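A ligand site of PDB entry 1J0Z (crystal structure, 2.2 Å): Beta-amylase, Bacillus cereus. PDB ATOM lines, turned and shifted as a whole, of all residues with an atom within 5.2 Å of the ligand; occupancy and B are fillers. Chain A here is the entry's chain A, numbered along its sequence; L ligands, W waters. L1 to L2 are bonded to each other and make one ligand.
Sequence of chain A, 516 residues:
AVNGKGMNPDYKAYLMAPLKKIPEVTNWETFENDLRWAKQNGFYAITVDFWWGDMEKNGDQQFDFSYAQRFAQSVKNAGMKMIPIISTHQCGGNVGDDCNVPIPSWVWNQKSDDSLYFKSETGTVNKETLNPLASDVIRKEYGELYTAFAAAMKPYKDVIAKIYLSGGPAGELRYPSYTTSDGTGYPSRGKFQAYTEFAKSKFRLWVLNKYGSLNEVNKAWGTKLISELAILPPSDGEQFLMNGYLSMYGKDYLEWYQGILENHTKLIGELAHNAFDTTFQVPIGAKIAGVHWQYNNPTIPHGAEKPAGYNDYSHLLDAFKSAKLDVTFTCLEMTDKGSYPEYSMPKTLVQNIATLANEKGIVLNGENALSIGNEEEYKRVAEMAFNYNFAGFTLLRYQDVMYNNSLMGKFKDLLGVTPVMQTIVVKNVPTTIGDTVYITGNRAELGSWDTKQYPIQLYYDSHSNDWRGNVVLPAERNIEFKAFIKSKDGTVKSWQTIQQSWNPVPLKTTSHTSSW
Water W3 lies within hydrogen-bond range of O of Val 95 (2.6 Å), O1 of LG2 L2 (2.6 Å) and OD2 of Asp 97 (2.7 Å).
Water W8 lies within hydrogen-bond range of O of Asn 368 (2.5 Å), OE1 of Glu 367 (2.8 Å), O1 of LIG L1 (2.8 Å) and OG1 of Thr 330 (3.0 Å).
Water W5 lies within hydrogen-bond range of an oxygen (O3) of LG2 L2, the side-chain amino group of Lys 287 and the backbone carbonyl oxygen of Ala 170.
Water W4 lies within hydrogen-bond range of O of Gln 90 (2.6 Å), O2 of LG2 L2 (2.9 Å), OD1 of Asp 97 (2.9 Å) and ND2 of Asn 94 (3.2 Å).
Water W1 lies within hydrogen-bond range of an oxygen (O5) of LG2 L2, the side-chain carboxylate of Asp 49 and the side-chain sulfur of Met 16.
Water W2 lies within hydrogen-bond range of an oxygen (O2) of LIG L1 (2.9 Å) and the backbone carbonyl oxygen of Ala 369 (3.2 Å).
O of Ala 17 sits at hydrogen-bond distance from NH1 of Arg 397 (3.0 Å).
The indole nitrogen (NE1) of Trp 51 lies within hydrogen-bond range of the backbone carbonyl oxygen (O) of Leu 19 (3.2 Å).
The side-chain hydroxyl (OG1) of Thr 330 lies within hydrogen-bond range of the backbone NH (N) of Ala 369, at 3.2 Å.
The side-chain carboxylate (OE2) of Glu 367 is in salt-bridge range of the side-chain amino group (NZ) of Lys 287.
OD1 of Asp 49 sits at hydrogen-bond distance from OG of Ser 87 (2.6 Å).
The side-chain carboxylate (OD1) of Asp 97 is in hydrogen-bond range of the backbone NH (N) of Asn 94.
A ring nitrogen (ND1) of His 89 is in hydrogen-bond range of the backbone NH of Gly 171.
OG1 of Thr 330 lies close to O of Glu 367 (3.5 Å).
The side-chain carboxylate (OE1) of Glu 172 sits close to an oxygen (O5) of LIG L1 (3.5 Å).
Leu 19 touches the ligand.
Trp 51 touches the ligand.
Ala 170 touches the ligand.
CD1 of Leu 396 touches O3 of LIG L1, 3.9 Å away.
Hydrophobic or aromatic side chains within 4 Å of the ligand: Met 16, Leu 19, Trp 51, His 89, Val 95, Ala 369 and Leu 396.
Within 4 Å of the ligand: Met 16, Leu 19, Asp 49, Trp 51, His 89, Val 95, Asp 97, Ala 170, Glu 172, Lys 287, Thr 330, Glu 367, Ala 369, Leu 396 and Arg 397.
A ring nitrogen (NE2) of His 89 sits at hydrogen-bond distance from an oxygen (O3) of LG2 L2 (2.9 Å).
NH2 of Arg 397 is in hydrogen-bond range of O4 of LG2 L2 (2.8 Å).
The side-chain amino group (NZ) of Lys 287 sits at hydrogen-bond distance from an oxygen (O6) of LIG L1, at 3.2 Å.
The side-chain carboxylate (OE1) of Glu 367 lies within hydrogen-bond range of an oxygen (O6) of LIG L1, 2.9 Å away.
SD of Met 16 sits at hydrogen-bond distance from O5 of LG2 L2.
An oxygen (O1) of LIG L1 is in hydrogen-bond range of the side-chain hydroxyl (OG1) of Thr 330 (3.2 Å).
An oxygen (O3) of LIG L1 is in hydrogen-bond range of the backbone carbonyl oxygen (O) of Val 95 (3.4 Å).
O of Ala 369 sits at hydrogen-bond distance from O2 of LIG L1 (2.6 Å).
An oxygen (O5) of LG2 L2 lies within hydrogen-bond range of the side-chain carboxylate (OD2) of Asp 49, 2.6 Å away.
An oxygen (O1) of LG2 L2 is in hydrogen-bond range of the side-chain carboxylate (OD2) of Asp 97.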
ATOM      1  N   MET A  16     -27.220 -11.172  -8.831  1.00  0.00           N
ATOM      2  CA  MET A  16     -26.724 -12.385  -9.440  1.00  0.00           C
ATOM      3  C   MET A  16     -27.704 -12.943 -10.451  1.00  0.00           C
ATOM      4  O   MET A  16     -28.901 -13.044 -10.181  1.00  0.00           O
ATOM      5  CB  MET A  16     -26.438 -13.445  -8.371  1.00  0.00           C
ATOM      6  CG  MET A  16     -25.051 -13.342  -7.762  1.00  0.00           C
ATOM      7  SD  MET A  16     -24.638 -14.771  -6.776  1.00  0.00           S
ATOM      8  CE  MET A  16     -24.143 -14.000  -5.259  1.00  0.00           C
ATOM      9  N   ALA A  17     -27.179 -13.299 -11.625  1.00  0.00           N
ATOM     10  CA  ALA A  17     -27.968 -13.874 -12.696  1.00  0.00           C
ATOM     11  C   ALA A  17     -28.283 -15.316 -12.358  1.00  0.00           C
ATOM     12  O   ALA A  17     -27.735 -15.870 -11.391  1.00  0.00           O
ATOM     13  CB  ALA A  17     -27.174 -13.820 -13.999  1.00  0.00           C
ATOM     14  N   LEU A  19     -28.333 -19.453 -12.621  1.00  0.00           N
ATOM     15  CA  LEU A  19     -27.242 -20.409 -12.826  1.00  0.00           C
ATOM     16  C   LEU A  19     -27.268 -20.989 -14.245  1.00  0.00           C
ATOM     17  O   LEU A  19     -26.233 -21.358 -14.801  1.00  0.00           O
ATOM     18  CB  LEU A  19     -27.349 -21.539 -11.802  1.00  0.00           C
ATOM     19  CG  LEU A  19     -26.310 -21.698 -10.693  1.00  0.00           C
ATOM     20  CD1 LEU A  19     -25.734 -20.370 -10.255  1.00  0.00           C
ATOM     21  CD2 LEU A  19     -26.955 -22.431  -9.529  1.00  0.00           C
ATOM     22  N   ASP A  49     -22.138 -16.095 -14.171  1.00  0.00           N
ATOM     23  CA  ASP A  49     -21.170 -17.169 -14.305  1.00  0.00           C
ATOM     24  C   ASP A  49     -21.060 -17.593 -15.770  1.00  0.00           C
ATOM     25  O   ASP A  49     -22.070 -17.828 -16.441  1.00  0.00           O
ATOM     26  CB  ASP A  49     -21.610 -18.405 -13.517  1.00  0.00           C
ATOM     27  CG  ASP A  49     -21.479 -18.231 -12.012  1.00  0.00           C
ATOM     28  OD1 ASP A  49     -20.369 -18.423 -11.476  1.00  0.00           O
ATOM     29  OD2 ASP A  49     -22.500 -17.900 -11.374  1.00  0.00           O
ATOM     30  N   TRP A  51     -19.503 -20.440 -17.471  1.00  0.00           N
ATOM     31  CA  TRP A  51     -18.945 -21.744 -17.198  1.00  0.00           C
ATOM     32  C   TRP A  51     -17.841 -22.235 -18.136  1.00  0.00           C
ATOM     33  O   TRP A  51     -18.005 -22.249 -19.353  1.00  0.00           O
ATOM     34  CB  TRP A  51     -20.074 -22.772 -17.113  1.00  0.00           C
ATOM     35  CG  TRP A  51     -21.135 -22.359 -16.142  1.00  0.00           C
ATOM     36  CD1 TRP A  51     -22.386 -21.907 -16.431  1.00  0.00           C
ATOM     37  CD2 TRP A  51     -21.010 -22.310 -14.706  1.00  0.00           C
ATOM     38  NE1 TRP A  51     -23.045 -21.565 -15.264  1.00  0.00           N
ATOM     39  CE2 TRP A  51     -22.220 -21.806 -14.195  1.00  0.00           C
ATOM     40  CE3 TRP A  51     -19.979 -22.631 -13.808  1.00  0.00           C
ATOM     41  CZ2 TRP A  51     -22.435 -21.619 -12.825  1.00  0.00           C
ATOM     42  CZ3 TRP A  51     -20.200 -22.457 -12.464  1.00  0.00           C
ATOM     43  CH2 TRP A  51     -21.418 -21.950 -11.983  1.00  0.00           C
ATOM     44  N   ILE A  85     -18.047 -13.752 -14.276  1.00  0.00           N
ATOM     45  CA  ILE A  85     -17.271 -14.614 -13.397  1.00  0.00           C
ATOM     46  C   ILE A  85     -16.735 -15.729 -14.292  1.00  0.00           C
ATOM     47  O   ILE A  85     -17.509 -16.486 -14.887  1.00  0.00           O
ATOM     48  CB  ILE A  85     -18.133 -15.233 -12.273  1.00  0.00           C
ATOM     49  CG1 ILE A  85     -18.856 -14.133 -11.490  1.00  0.00           C
ATOM     50  CG2 ILE A  85     -17.258 -16.066 -11.335  1.00  0.00           C
ATOM     51  CD1 ILE A  85     -19.872 -14.637 -10.495  1.00  0.00           C
ATOM     52  N   SER A  87     -15.940 -18.763 -14.455  1.00  0.00           N
ATOM     53  CA  SER A  87     -16.156 -19.936 -13.634  1.00  0.00           C
ATOM     54  C   SER A  87     -15.458 -21.207 -14.074  1.00  0.00           C
ATOM     55  O   SER A  87     -16.006 -22.013 -14.819  1.00  0.00           O
ATOM     56  CB  SER A  87     -17.644 -20.170 -13.462  1.00  0.00           C
ATOM     57  OG  SER A  87     -18.246 -19.043 -12.847  1.00  0.00           O
ATOM     58  N   HIS A  89     -15.005 -23.568 -12.277  1.00  0.00           N
ATOM     59  CA  HIS A  89     -15.493 -24.561 -11.318  1.00  0.00           C
ATOM     60  C   HIS A  89     -16.767 -25.178 -11.873  1.00  0.00           C
ATOM     61  O   HIS A  89     -17.369 -24.661 -12.829  1.00  0.00           O
ATOM     62  CB  HIS A  89     -15.729 -23.928  -9.927  1.00  0.00           C
ATOM     63  CG  HIS A  89     -16.823 -22.901  -9.889  1.00  0.00           C
ATOM     64  ND1 HIS A  89     -16.588 -21.562 -10.112  1.00  0.00           N
ATOM     65  CD2 HIS A  89     -18.156 -23.018  -9.660  1.00  0.00           C
ATOM     66  CE1 HIS A  89     -17.724 -20.900 -10.038  1.00  0.00           C
ATOM     67  NE2 HIS A  89     -18.684 -21.755  -9.759  1.00  0.00           N
ATOM     68  N   GLN A  90     -17.179 -26.293 -11.276  1.00  0.00           N
ATOM     69  CA  GLN A  90     -18.379 -26.991 -11.705  1.00  0.00           C
ATOM     70  C   GLN A  90     -19.668 -26.435 -11.126  1.00  0.00           C
ATOM     71  O   GLN A  90     -19.715 -26.028  -9.961  1.00  0.00           O
ATOM     72  CB  GLN A  90     -18.258 -28.466 -11.341  1.00  0.00           C
ATOM     73  CG  GLN A  90     -19.522 -29.262 -11.546  1.00  0.00           C
ATOM     74  CD  GLN A  90     -19.445 -30.629 -10.956  1.00  0.00           C
ATOM     75  OE1 GLN A  90     -18.423 -31.312 -11.074  1.00  0.00           O
ATOM     76  NE2 GLN A  90     -20.507 -31.041 -10.288  1.00  0.00           N
ATOM     77  N   CYS A  91     -20.717 -26.405 -11.941  1.00  0.00           N
ATOM     78  CA  CYS A  91     -22.011 -25.942 -11.495  1.00  0.00           C
ATOM     79  C   CYS A  91     -22.781 -27.218 -11.194  1.00  0.00           C
ATOM     80  O   CYS A  91     -22.803 -28.138 -12.003  1.00  0.00           O
ATOM     81  CB  CYS A  91     -22.736 -25.167 -12.592  1.00  0.00           C
ATOM     82  SG  CYS A  91     -24.111 -24.154 -11.974  1.00  0.00           S
ATOM     83  N   ASN A  94     -23.461 -28.255  -5.161  1.00  0.00           N
ATOM     84  CA  ASN A  94     -23.393 -27.402  -3.972  1.00  0.00           C
ATOM     85  C   ASN A  94     -24.776 -26.852  -3.669  1.00  0.00           C
ATOM     86  O   ASN A  94     -25.730 -27.088  -4.409  1.00  0.00           O
ATOM     87  CB  ASN A  94     -22.390 -26.257  -4.187  1.00  0.00           C
ATOM     88  CG  ASN A  94     -20.939 -26.730  -4.143  1.00  0.00           C
ATOM     89  OD1 ASN A  94     -20.594 -27.676  -3.420  1.00  0.00           O
ATOM     90  ND2 ASN A  94     -20.085 -26.058  -4.893  1.00  0.00           N
ATOM     91  N   VAL A  95     -24.879 -26.107  -2.565  1.00  0.00           N
ATOM     92  CA  VAL A  95     -26.161 -25.533  -2.152  1.00  0.00           C
ATOM     93  C   VAL A  95     -26.719 -24.519  -3.169  1.00  0.00           C
ATOM     94  O   VAL A  95     -26.001 -23.622  -3.621  1.00  0.00           O
ATOM     95  CB  VAL A  95     -26.072 -24.864  -0.756  1.00  0.00           C
ATOM     96  CG1 VAL A  95     -25.110 -23.674  -0.780  1.00  0.00           C
ATOM     97  CG2 VAL A  95     -27.454 -24.443  -0.277  1.00  0.00           C
ATOM     98  N   ASP A  97     -27.518 -25.157  -6.171  1.00  0.00           N
ATOM     99  CA  ASP A  97     -27.100 -25.483  -7.520  1.00  0.00           C
ATOM    100  C   ASP A  97     -28.151 -26.174  -8.395  1.00  0.00           C
ATOM    101  O   ASP A  97     -28.246 -27.405  -8.429  1.00  0.00           O
ATOM    102  CB  ASP A  97     -25.794 -26.288  -7.508  1.00  0.00           C
ATOM    103  CG  ASP A  97     -24.549 -25.413  -7.454  1.00  0.00           C
ATOM    104  OD1 ASP A  97     -23.432 -25.950  -7.340  1.00  0.00           O
ATOM    105  OD2 ASP A  97     -24.665 -24.168  -7.552  1.00  0.00           O
ATOM    106  N   ALA A 170     -17.330 -23.697  -5.950  1.00  0.00           N
ATOM    107  CA  ALA A 170     -18.362 -22.668  -5.925  1.00  0.00           C
ATOM    108  C   ALA A 170     -17.829 -21.261  -6.215  1.00  0.00           C
ATOM    109  O   ALA A 170     -18.479 -20.264  -5.882  1.00  0.00           O
ATOM    110  CB  ALA A 170     -19.101 -22.685  -4.590  1.00  0.00           C
ATOM    111  N   GLY A 171     -16.662 -21.170  -6.840  1.00  0.00           N
ATOM    112  CA  GLY A 171     -16.078 -19.885  -7.158  1.00  0.00           C
ATOM    113  C   GLY A 171     -15.388 -19.193  -5.993  1.00  0.00           C
ATOM    114  O   GLY A 171     -15.037 -18.006  -6.077  1.00  0.00           O
ATOM    115  N   GLU A 172     -15.141 -19.938  -4.920  1.00  0.00           N
ATOM    116  CA  GLU A 172     -14.500 -19.422  -3.722  1.00  0.00           C
ATOM    117  C   GLU A 172     -13.089 -19.978  -3.569  1.00  0.00           C
ATOM    118  O   GLU A 172     -12.826 -21.117  -3.954  1.00  0.00           O
ATOM    119  CB  GLU A 172     -15.350 -19.775  -2.498  1.00  0.00           C
ATOM    120  CG  GLU A 172     -16.752 -19.223  -2.579  1.00  0.00           C
ATOM    121  CD  GLU A 172     -17.701 -19.840  -1.556  1.00  0.00           C
ATOM    122  OE1 GLU A 172     -18.436 -19.082  -0.892  1.00  0.00           O
ATOM    123  OE2 GLU A 172     -17.741 -21.087  -1.439  1.00  0.00           O
ATOM    124  N   LYS A 287     -13.321 -14.456  -4.348  1.00  0.00           N
ATOM    125  CA  LYS A 287     -14.147 -14.693  -3.167  1.00  0.00           C
ATOM    126  C   LYS A 287     -13.574 -15.603  -2.079  1.00  0.00           C
ATOM    127  O   LYS A 287     -12.907 -16.604  -2.361  1.00  0.00           O
ATOM    128  CB  LYS A 287     -15.505 -15.269  -3.604  1.00  0.00           C
ATOM    129  CG  LYS A 287     -16.210 -14.489  -4.690  1.00  0.00           C
ATOM    130  CD  LYS A 287     -17.525 -15.141  -5.062  1.00  0.00           C
ATOM    131  CE  LYS A 287     -18.169 -14.453  -6.252  1.00  0.00           C
ATOM    132  NZ  LYS A 287     -19.519 -15.005  -6.573  1.00  0.00           N
ATOM    133  N   THR A 330     -19.068 -13.449   2.093  1.00  0.00           N
ATOM    134  CA  THR A 330     -20.500 -13.700   2.201  1.00  0.00           C
ATOM    135  C   THR A 330     -20.996 -13.691   3.670  1.00  0.00           C
ATOM    136  O   THR A 330     -20.297 -13.212   4.561  1.00  0.00           O
ATOM    137  CB  THR A 330     -20.870 -15.032   1.492  1.00  0.00           C
ATOM    138  OG1 THR A 330     -22.285 -15.135   1.355  1.00  0.00           O
ATOM    139  CG2 THR A 330     -20.334 -16.228   2.269  1.00  0.00           C
ATOM    140  N   GLU A 367     -21.917 -10.425   0.028  1.00  0.00           N
ATOM    141  CA  GLU A 367     -23.015 -11.212  -0.548  1.00  0.00           C
ATOM    142  C   GLU A 367     -23.804 -11.836   0.602  1.00  0.00           C
ATOM    143  O   GLU A 367     -23.347 -11.874   1.749  1.00  0.00           O
ATOM    144  CB  GLU A 367     -22.472 -12.381  -1.379  1.00  0.00           C
ATOM    145  CG  GLU A 367     -21.828 -12.055  -2.708  1.00  0.00           C
ATOM    146  CD  GLU A 367     -21.261 -13.297  -3.386  1.00  0.00           C
ATOM    147  OE1 GLU A 367     -21.555 -14.429  -2.942  1.00  0.00           O
ATOM    148  OE2 GLU A 367     -20.493 -13.144  -4.360  1.00  0.00           O
ATOM    149  N   ASN A 368     -24.994 -12.338   0.278  1.00  0.00           N
ATOM    150  CA  ASN A 368     -25.818 -13.041   1.250  1.00  0.00           C
ATOM    151  C   ASN A 368     -25.590 -14.516   0.922  1.00  0.00           C
ATOM    152  O   ASN A 368     -25.539 -14.899  -0.245  1.00  0.00           O
ATOM    153  CB  ASN A 368     -27.292 -12.671   1.115  1.00  0.00           C
ATOM    154  CG  ASN A 368     -27.808 -12.784  -0.300  1.00  0.00           C
ATOM    155  OD1 ASN A 368     -27.435 -11.992  -1.168  1.00  0.00           O
ATOM    156  ND2 ASN A 368     -28.654 -13.753  -0.554  1.00  0.00           N
ATOM    157  N   ALA A 369     -25.389 -15.321   1.965  1.00  0.00           N
ATOM    158  CA  ALA A 369     -25.146 -16.743   1.816  1.00  0.00           C
ATOM    159  C   ALA A 369     -26.328 -17.529   1.267  1.00  0.00           C
ATOM    160  O   ALA A 369     -26.153 -18.438   0.461  1.00  0.00           O
ATOM    161  CB  ALA A 369     -24.705 -17.332   3.151  1.00  0.00           C
ATOM    162  N   LEU A 370     -27.534 -17.191   1.715  1.00  0.00           N
ATOM    163  CA  LEU A 370     -28.733 -17.902   1.281  1.00  0.00           C
ATOM    164  C   LEU A 370     -29.769 -16.913   0.797  1.00  0.00           C
ATOM    165  O   LEU A 370     -29.630 -15.714   1.020  1.00  0.00           O
ATOM    166  CB  LEU A 370     -29.322 -18.715   2.443  1.00  0.00           C
ATOM    167  CG  LEU A 370     -28.451 -19.788   3.097  1.00  0.00           C
ATOM    168  CD1 LEU A 370     -29.193 -20.359   4.295  1.00  0.00           C
ATOM    169  CD2 LEU A 370     -28.125 -20.883   2.093  1.00  0.00           C
ATOM    170  N   LEU A 396     -28.079 -12.469  -3.990  1.00  0.00           N
ATOM    171  CA  LEU A 396     -28.281 -13.802  -4.527  1.00  0.00           C
ATOM    172  C   LEU A 396     -29.745 -14.076  -4.169  1.00  0.00           C
ATOM    173  O   LEU A 396     -30.108 -14.066  -2.996  1.00  0.00           O
ATOM    174  CB  LEU A 396     -27.330 -14.787  -3.813  1.00  0.00           C
ATOM    175  CG  LEU A 396     -27.273 -16.274  -4.178  1.00  0.00           C
ATOM    176  CD1 LEU A 396     -25.923 -16.859  -3.764  1.00  0.00           C
ATOM    177  CD2 LEU A 396     -28.420 -17.041  -3.511  1.00  0.00           C
ATOM    178  N   ARG A 397     -30.617 -14.292  -5.163  1.00  0.00           N
ATOM    179  CA  ARG A 397     -30.261 -14.313  -6.585  1.00  0.00           C
ATOM    180  C   ARG A 397     -31.448 -13.792  -7.398  1.00  0.00           C
ATOM    181  O   ARG A 397     -32.566 -13.723  -6.886  1.00  0.00           O
ATOM    182  CB  ARG A 397     -29.945 -15.763  -6.984  1.00  0.00           C
ATOM    183  CG  ARG A 397     -29.383 -15.956  -8.377  1.00  0.00           C
ATOM    184  CD  ARG A 397     -29.182 -17.444  -8.677  1.00  0.00           C
ATOM    185  NE  ARG A 397     -28.157 -18.062  -7.838  1.00  0.00           N
ATOM    186  CZ  ARG A 397     -26.849 -18.007  -8.067  1.00  0.00           C
ATOM    187  NH1 ARG A 397     -26.365 -17.342  -9.119  1.00  0.00           N
ATOM    188  NH2 ARG A 397     -26.001 -18.644  -7.267  1.00  0.00           N
HETATM  189  C1  LIG L   1     -23.654 -19.259  -1.663  1.00  0.00           C
HETATM  190  C2  LIG L   1     -23.416 -20.138  -2.869  1.00  0.00           C
HETATM  191  C3  LIG L   1     -22.578 -19.360  -3.898  1.00  0.00           C
HETATM  192  C4  LIG L   1     -21.265 -18.930  -3.225  1.00  0.00           C
HETATM  193  C5  LIG L   1     -20.364 -18.100  -4.121  1.00  0.00           C
HETATM  194  C6  LIG L   1     -22.313 -18.856  -1.076  1.00  0.00           C
HETATM  195  O1  LIG L   1     -22.510 -18.017   0.005  1.00  0.00           O
HETATM  196  O2  LIG L   1     -24.414 -19.963  -0.696  1.00  0.00           O
HETATM  197  O3  LIG L   1     -24.663 -20.542  -3.419  1.00  0.00           O
HETATM  198  O4  LIG L   1     -22.289 -20.213  -5.023  1.00  0.00           O
HETATM  199  O5  LIG L   1     -21.547 -18.141  -2.050  1.00  0.00           O
HETATM  200  O6  LIG L   1     -20.941 -16.830  -4.406  1.00  0.00           O
HETATM  201  C1  LG2 L   2     -23.221 -20.232  -6.067  1.00  0.00           C
HETATM  202  C2  LG2 L   2     -22.909 -21.393  -6.999  1.00  0.00           C
HETATM  203  C3  LG2 L   2     -21.557 -21.143  -7.650  1.00  0.00           C
HETATM  204  C4  LG2 L   2     -21.606 -19.825  -8.420  1.00  0.00           C
HETATM  205  C5  LG2 L   2     -22.046 -18.667  -7.503  1.00  0.00           C
HETATM  206  C6  LG2 L   2     -22.334 -17.384  -8.263  1.00  0.00           C
HETATM  207  O1  LG2 L   2     -22.869 -22.597  -6.248  1.00  0.00           O
HETATM  208  O2  LG2 L   2     -21.223 -22.200  -8.533  1.00  0.00           O
HETATM  209  O3  LG2 L   2     -20.317 -19.556  -8.953  1.00  0.00           O
HETATM  210  O4  LG2 L   2     -23.262 -19.005  -6.798  1.00  0.00           O
HETATM  211  O5  LG2 L   2     -23.541 -17.482  -9.010  1.00  0.00           O
HETATM  212  O   HOH W   1     -23.817 -14.937 -10.329  1.00  0.00           O
HETATM  213  O   HOH W   2     -27.074 -20.555  -1.736  1.00  0.00           O
HETATM  214  O   HOH W   3     -25.438 -22.313  -5.761  1.00  0.00           O
HETATM  215  O   HOH W   4     -20.758 -24.936  -7.812  1.00  0.00           O
HETATM  216  O   HOH W   5     -18.676 -17.693  -7.550  1.00  0.00           O
HETATM  217  O   HOH W   6     -27.024 -20.218  -5.072  1.00  0.00           O
HETATM  218  O   HOH W   7     -22.860 -23.220  -3.582  1.00  0.00           O
HETATM  219  O   HOH W   8     -23.455 -15.727  -1.339  1.00  0.00           O
